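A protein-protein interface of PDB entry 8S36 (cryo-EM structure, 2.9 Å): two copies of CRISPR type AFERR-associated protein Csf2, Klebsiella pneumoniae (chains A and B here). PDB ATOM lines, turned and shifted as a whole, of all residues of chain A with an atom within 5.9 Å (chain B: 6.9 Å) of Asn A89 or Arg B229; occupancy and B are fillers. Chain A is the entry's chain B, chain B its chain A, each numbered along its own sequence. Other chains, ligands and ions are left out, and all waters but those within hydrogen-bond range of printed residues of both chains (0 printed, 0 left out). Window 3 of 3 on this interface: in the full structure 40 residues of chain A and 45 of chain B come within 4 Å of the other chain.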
ATOM      1  N   ASP A  75      14.122   0.917  35.124  1.00  0.00           N
ATOM      2  CA  ASP A  75      15.087   0.472  34.134  1.00  0.00           C
ATOM      3  C   ASP A  75      16.345   1.337  34.196  1.00  0.00           C
ATOM      4  O   ASP A  75      16.424   2.323  34.933  1.00  0.00           O
ATOM      5  CB  ASP A  75      14.477   0.505  32.731  1.00  0.00           C
ATOM      6  CG  ASP A  75      13.935   1.872  32.354  1.00  0.00           C
ATOM      7  OD1 ASP A  75      14.699   2.859  32.401  1.00  0.00           O
ATOM      8  OD2 ASP A  75      12.739   1.958  32.005  1.00  0.00           O
ATOM      9  N   ALA A  77      17.583   3.224  31.819  1.00  0.00           N
ATOM     10  CA  ALA A  77      17.328   4.543  31.253  1.00  0.00           C
ATOM     11  C   ALA A  77      16.780   5.485  32.312  1.00  0.00           C
ATOM     12  O   ALA A  77      17.184   6.650  32.390  1.00  0.00           O
ATOM     13  CB  ALA A  77      16.360   4.435  30.075  1.00  0.00           C
ATOM     14  N   ASP A  87      19.316  10.569  28.712  1.00  0.00           N
ATOM     15  CA  ASP A  87      18.387   9.545  28.250  1.00  0.00           C
ATOM     16  C   ASP A  87      19.116   8.663  27.245  1.00  0.00           C
ATOM     17  O   ASP A  87      19.400   9.092  26.122  1.00  0.00           O
ATOM     18  CB  ASP A  87      17.144  10.176  27.628  1.00  0.00           C
ATOM     19  CG  ASP A  87      15.998   9.193  27.492  1.00  0.00           C
ATOM     20  OD1 ASP A  87      15.506   8.707  28.531  1.00  0.00           O
ATOM     21  OD2 ASP A  87      15.590   8.909  26.345  1.00  0.00           O
ATOM     22  N   ILE A  88      19.417   7.431  27.651  1.00  0.00           N
ATOM     23  CA  ILE A  88      20.063   6.490  26.744  1.00  0.00           C
ATOM     24  C   ILE A  88      19.102   6.069  25.641  1.00  0.00           C
ATOM     25  O   ILE A  88      19.505   5.855  24.491  1.00  0.00           O
ATOM     26  CB  ILE A  88      20.603   5.284  27.536  1.00  0.00           C
ATOM     27  CG1 ILE A  88      19.460   4.481  28.169  1.00  0.00           C
ATOM     28  CG2 ILE A  88      21.554   5.774  28.612  1.00  0.00           C
ATOM     29  CD1 ILE A  88      19.922   3.299  28.999  1.00  0.00           C
ATOM     30  N   ASN A  89      17.816   5.945  25.972  1.00  0.00           N
ATOM     31  CA  ASN A  89      16.827   5.529  24.984  1.00  0.00           C
ATOM     32  C   ASN A  89      16.643   6.585  23.904  1.00  0.00           C
ATOM     33  O   ASN A  89      16.402   6.253  22.737  1.00  0.00           O
ATOM     34  CB  ASN A  89      15.493   5.241  25.671  1.00  0.00           C
ATOM     35  CG  ASN A  89      15.585   4.103  26.663  1.00  0.00           C
ATOM     36  OD1 ASN A  89      16.606   3.424  26.752  1.00  0.00           O
ATOM     37  ND2 ASN A  89      14.514   3.890  27.419  1.00  0.00           N
ATOM     38  N   GLY A  90      16.737   7.859  24.273  1.00  0.00           N
ATOM     39  CA  GLY A  90      16.306   8.927  23.403  1.00  0.00           C
ATOM     40  C   GLY A  90      14.807   9.110  23.354  1.00  0.00           C
ATOM     41  O   GLY A  90      14.325   9.938  22.570  1.00  0.00           O
ATOM     42  N   GLU A  91      14.055   8.366  24.167  1.00  0.00           N
ATOM     43  CA  GLU A  91      12.604   8.476  24.207  1.00  0.00           C
ATOM     44  C   GLU A  91      12.124   9.589  25.127  1.00  0.00           C
ATOM     45  O   GLU A  91      10.933   9.919  25.094  1.00  0.00           O
ATOM     46  CB  GLU A  91      11.992   7.145  24.654  1.00  0.00           C
ATOM     47  CG  GLU A  91      12.315   6.758  26.099  1.00  0.00           C
ATOM     48  CD  GLU A  91      11.272   7.229  27.103  1.00  0.00           C
ATOM     49  OE1 GLU A  91      10.091   7.382  26.728  1.00  0.00           O
ATOM     50  OE2 GLU A  91      11.642   7.452  28.275  1.00  0.00           O
ATOM     51  N   ALA A  92      13.005  10.137  25.965  1.00  0.00           N
ATOM     52  CA  ALA A  92      12.686  11.333  26.733  1.00  0.00           C
ATOM     53  C   ALA A  92      12.012  12.367  25.844  1.00  0.00           C
ATOM     54  O   ALA A  92      12.473  12.645  24.734  1.00  0.00           O
ATOM     55  CB  ALA A  92      13.958  11.915  27.353  1.00  0.00           C
ATOM     56  N   ALA A 342       9.356   5.987  32.440  1.00  0.00           N
ATOM     57  CA  ALA A 342       9.461   6.595  31.118  1.00  0.00           C
ATOM     58  C   ALA A 342       8.147   7.257  30.721  1.00  0.00           C
ATOM     59  O   ALA A 342       8.097   8.463  30.481  1.00  0.00           O
ATOM     60  CB  ALA A 342       9.860   5.552  30.088  1.00  0.00           C
ATOM     61  N   ARG B 167      22.142  -4.820  30.290  1.00  0.00           N
ATOM     62  CA  ARG B 167      22.005  -3.628  29.467  1.00  0.00           C
ATOM     63  C   ARG B 167      23.048  -2.586  29.849  1.00  0.00           C
ATOM     64  O   ARG B 167      23.535  -1.850  28.986  1.00  0.00           O
ATOM     65  CB  ARG B 167      20.591  -3.072  29.628  1.00  0.00           C
ATOM     66  CG  ARG B 167      20.265  -1.842  28.813  1.00  0.00           C
ATOM     67  CD  ARG B 167      18.895  -1.315  29.204  1.00  0.00           C
ATOM     68  NE  ARG B 167      18.533  -0.097  28.491  1.00  0.00           N
ATOM     69  CZ  ARG B 167      17.315   0.426  28.477  1.00  0.00           C
ATOM     70  NH1 ARG B 167      16.311  -0.135  29.133  1.00  0.00           N
ATOM     71  NH2 ARG B 167      17.096   1.541  27.788  1.00  0.00           N
ATOM     72  N   LEU B 171      25.803  -1.321  27.278  1.00  0.00           N
ATOM     73  CA  LEU B 171      25.964   0.094  26.984  1.00  0.00           C
ATOM     74  C   LEU B 171      27.393   0.539  27.238  1.00  0.00           C
ATOM     75  O   LEU B 171      27.907   1.395  26.513  1.00  0.00           O
ATOM     76  CB  LEU B 171      24.980   0.911  27.824  1.00  0.00           C
ATOM     77  CG  LEU B 171      25.125   2.436  27.897  1.00  0.00           C
ATOM     78  CD1 LEU B 171      23.782   3.026  28.261  1.00  0.00           C
ATOM     79  CD2 LEU B 171      26.165   2.899  28.920  1.00  0.00           C
ATOM     80  N   GLU B 174      29.322  -0.789  24.254  1.00  0.00           N
ATOM     81  CA  GLU B 174      29.035   0.067  23.110  1.00  0.00           C
ATOM     82  C   GLU B 174      29.766   1.394  23.232  1.00  0.00           C
ATOM     83  O   GLU B 174      30.303   1.906  22.244  1.00  0.00           O
ATOM     84  CB  GLU B 174      27.529   0.298  22.992  1.00  0.00           C
ATOM     85  CG  GLU B 174      26.779  -0.817  22.286  1.00  0.00           C
ATOM     86  CD  GLU B 174      25.316  -0.485  22.067  1.00  0.00           C
ATOM     87  OE1 GLU B 174      24.878   0.598  22.509  1.00  0.00           O
ATOM     88  OE2 GLU B 174      24.604  -1.306  21.453  1.00  0.00           O
ATOM     89  N   ARG B 221      28.805   6.017  12.999  1.00  0.00           N
ATOM     90  CA  ARG B 221      29.257   5.273  14.170  1.00  0.00           C
ATOM     91  C   ARG B 221      28.467   5.648  15.422  1.00  0.00           C
ATOM     92  O   ARG B 221      28.200   4.788  16.270  1.00  0.00           O
ATOM     93  CB  ARG B 221      30.753   5.513  14.388  1.00  0.00           C
ATOM     94  CG  ARG B 221      31.367   4.729  15.545  1.00  0.00           C
ATOM     95  CD  ARG B 221      31.440   3.238  15.260  1.00  0.00           C
ATOM     96  NE  ARG B 221      31.542   2.464  16.492  1.00  0.00           N
ATOM     97  CZ  ARG B 221      30.518   2.164  17.279  1.00  0.00           C
ATOM     98  NH1 ARG B 221      29.287   2.561  17.000  1.00  0.00           N
ATOM     99  NH2 ARG B 221      30.734   1.448  18.379  1.00  0.00           N
ATOM    100  N   LYS B 222      28.079   6.919  15.561  1.00  0.00           N
ATOM    101  CA  LYS B 222      27.306   7.350  16.721  1.00  0.00           C
ATOM    102  C   LYS B 222      25.805   7.180  16.537  1.00  0.00           C
ATOM    103  O   LYS B 222      25.038   7.586  17.417  1.00  0.00           O
ATOM    104  CB  LYS B 222      27.615   8.815  17.046  1.00  0.00           C
ATOM    105  CG  LYS B 222      27.926   9.068  18.511  1.00  0.00           C
ATOM    106  CD  LYS B 222      28.144  10.547  18.788  1.00  0.00           C
ATOM    107  CE  LYS B 222      29.470  11.030  18.224  1.00  0.00           C
ATOM    108  NZ  LYS B 222      29.799  12.411  18.667  1.00  0.00           N
ATOM    109  N   ASP B 223      25.372   6.597  15.420  1.00  0.00           N
ATOM    110  CA  ASP B 223      24.016   6.078  15.302  1.00  0.00           C
ATOM    111  C   ASP B 223      23.967   4.559  15.385  1.00  0.00           C
ATOM    112  O   ASP B 223      22.909   4.003  15.697  1.00  0.00           O
ATOM    113  CB  ASP B 223      23.389   6.527  13.977  1.00  0.00           C
ATOM    114  CG  ASP B 223      21.916   6.173  13.878  1.00  0.00           C
ATOM    115  OD1 ASP B 223      21.280   5.966  14.933  1.00  0.00           O
ATOM    116  OD2 ASP B 223      21.396   6.100  12.745  1.00  0.00           O
ATOM    117  N   LYS B 225      25.225   2.997  17.717  1.00  0.00           N
ATOM    118  CA  LYS B 225      25.030   2.745  19.141  1.00  0.00           C
ATOM    119  C   LYS B 225      23.535   2.684  19.421  1.00  0.00           C
ATOM    120  O   LYS B 225      22.857   3.716  19.433  1.00  0.00           O
ATOM    121  CB  LYS B 225      25.695   3.837  19.973  1.00  0.00           C
ATOM    122  CG  LYS B 225      27.166   4.087  19.645  1.00  0.00           C
ATOM    123  CD  LYS B 225      27.657   5.396  20.251  1.00  0.00           C
ATOM    124  CE  LYS B 225      27.929   5.261  21.739  1.00  0.00           C
ATOM    125  NZ  LYS B 225      28.564   6.485  22.300  1.00  0.00           N
ATOM    126  N   GLN B 226      23.012   1.476  19.635  1.00  0.00           N
ATOM    127  CA  GLN B 226      21.573   1.274  19.722  1.00  0.00           C
ATOM    128  C   GLN B 226      21.056   1.204  21.151  1.00  0.00           C
ATOM    129  O   GLN B 226      19.835   1.210  21.344  1.00  0.00           O
ATOM    130  CB  GLN B 226      21.179  -0.017  18.993  1.00  0.00           C
ATOM    131  CG  GLN B 226      21.315   0.047  17.481  1.00  0.00           C
ATOM    132  CD  GLN B 226      20.314   0.986  16.841  1.00  0.00           C
ATOM    133  OE1 GLN B 226      19.138   1.002  17.209  1.00  0.00           O
ATOM    134  NE2 GLN B 226      20.774   1.775  15.878  1.00  0.00           N
ATOM    135  N   GLU B 227      21.934   1.138  22.152  1.00  0.00           N
ATOM    136  CA  GLU B 227      21.492   1.260  23.538  1.00  0.00           C
ATOM    137  C   GLU B 227      21.496   2.719  23.988  1.00  0.00           C
ATOM    138  O   GLU B 227      20.462   3.248  24.411  1.00  0.00           O
ATOM    139  CB  GLU B 227      22.380   0.407  24.451  1.00  0.00           C
ATOM    140  CG  GLU B 227      21.896   0.313  25.893  1.00  0.00           C
ATOM    141  CD  GLU B 227      20.449  -0.124  26.004  1.00  0.00           C
ATOM    142  OE1 GLU B 227      20.115  -1.216  25.499  1.00  0.00           O
ATOM    143  OE2 GLU B 227      19.644   0.628  26.593  1.00  0.00           O
ATOM    144  N   SER B 228      22.648   3.376  23.902  1.00  0.00           N
ATOM    145  CA  SER B 228      22.767   4.817  24.064  1.00  0.00           C
ATOM    146  C   SER B 228      23.088   5.455  22.720  1.00  0.00           C
ATOM    147  O   SER B 228      23.456   4.779  21.755  1.00  0.00           O
ATOM    148  CB  SER B 228      23.848   5.163  25.094  1.00  0.00           C
ATOM    149  OG  SER B 228      25.116   4.687  24.679  1.00  0.00           O
ATOM    150  N   ARG B 229      22.951   6.780  22.667  1.00  0.00           N
ATOM    151  CA  ARG B 229      23.376   7.560  21.511  1.00  0.00           C
ATOM    152  C   ARG B 229      24.604   8.414  21.777  1.00  0.00           C
ATOM    153  O   ARG B 229      25.390   8.644  20.856  1.00  0.00           O
ATOM    154  CB  ARG B 229      22.236   8.468  21.032  1.00  0.00           C
ATOM    155  CG  ARG B 229      21.000   7.711  20.568  1.00  0.00           C
ATOM    156  CD  ARG B 229      19.986   7.539  21.687  1.00  0.00           C
ATOM    157  NE  ARG B 229      18.868   6.692  21.285  1.00  0.00           N
ATOM    158  CZ  ARG B 229      18.839   5.369  21.392  1.00  0.00           C
ATOM    159  NH1 ARG B 229      19.865   4.687  21.878  1.00  0.00           N
ATOM    160  NH2 ARG B 229      17.751   4.711  21.000  1.00  0.00           N
ATOM    161  N   GLU B 230      24.783   8.884  23.008  1.00  0.00           N
ATOM    162  CA  GLU B 230      25.924   9.698  23.400  1.00  0.00           C
ATOM    163  C   GLU B 230      26.706   8.988  24.494  1.00  0.00           C
ATOM    164  O   GLU B 230      26.122   8.335  25.364  1.00  0.00           O
ATOM    165  CB  GLU B 230      25.474  11.084  23.885  1.00  0.00           C
ATOM    166  CG  GLU B 230      26.595  11.966  24.431  1.00  0.00           C
ATOM    167  CD  GLU B 230      27.788  12.060  23.495  1.00  0.00           C
ATOM    168  OE1 GLU B 230      27.589  11.980  22.264  1.00  0.00           O
ATOM    169  OE2 GLU B 230      28.924  12.211  23.991  1.00  0.00           O
ATOM    170  N   SER B 231      28.028   9.119  24.447  1.00  0.00           N
ATOM    171  CA  SER B 231      28.874   8.556  25.489  1.00  0.00           C
ATOM    172  C   SER B 231      28.558   9.218  26.823  1.00  0.00           C
ATOM    173  O   SER B 231      28.638  10.443  26.952  1.00  0.00           O
ATOM    174  CB  SER B 231      30.347   8.748  25.132  1.00  0.00           C
ATOM    175  OG  SER B 231      30.653   8.141  23.890  1.00  0.00           O
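The backbone carbonyl oxygen (O) of Ile A88 lies within hydrogen-bond range of the guanidinium group (NH1) of Arg B229 (2.9 Å). The guanidinium group (NH2) of Arg B229 is in hydrogen-bond range of the backbone carbonyl oxygen (O) of Asn A89, at 2.7 Å. O of Glu B227 sits close to O of Ile A88 (2.8 Å). The side-chain amide oxygen (OD1) of Asn A89 lies close to the guanidinium group (NH2) of Arg B167, at 2.2 Å.
The side-chain carboxylate (OE2) of Glu B227 lies within salt-bridge range of the guanidinium group (NH2) of Arg B167 (3.0 Å). OE1 of Glu B174 lies within hydrogen-bond range of N of Glu B227 (3.0 Å). O of Glu B227 is in hydrogen-bond range of NH1 of Arg B229 (3.0 Å). OD1 of Asp A75 is in hydrogen-bond range of N of Ala A77, at 3.0 Å. OD2 of Asp A87 is in hydrogen-bond range of N of Gly A90.
Among the printed residues, pairs that only touch across the chains: Ile A88 with Ser B228, Ile A88 with Arg B167, Ile A88 with Leu B171, Ala A77 with Arg B167 and Gly A90 with Arg B229.
Of the printed residues of chain B, Ala A77 touches Arg B167. Printed residues of chain B within 4 Å of Ile A88: Arg B167 (3.5 Å), Leu B171 (3.6 Å), Glu B227 (2.8 Å), Ser B228 (3.4 Å) and Arg B229 (2.9 Å). Of chain B, only Arg B167 and Arg B229 come within 4 Å of Asn A89. Printed residues of chain A within 4 Å of Glu B227: Ile A88 (2.8 Å). Printed residues of chain A within 4 Å of Ser B228: Ile A88 (3.4 Å). Arg B229 touches just these residues of chain A: Ile A88, Asn A89 and Gly A90. The nearest residue of chain A that does not touch Arg B229 is Asp A87 (4.7 Å).
Hydrophobic or aromatic side chains of chain B within 4 Å of the printed part of chain A: Leu B171. Among the printed residues, 9 pairs touch across the chains.
No position is printed for both chains. Of the 9 pairs that touch across the chains among the printed residues, none has its exchanged pair printed and touching as well.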
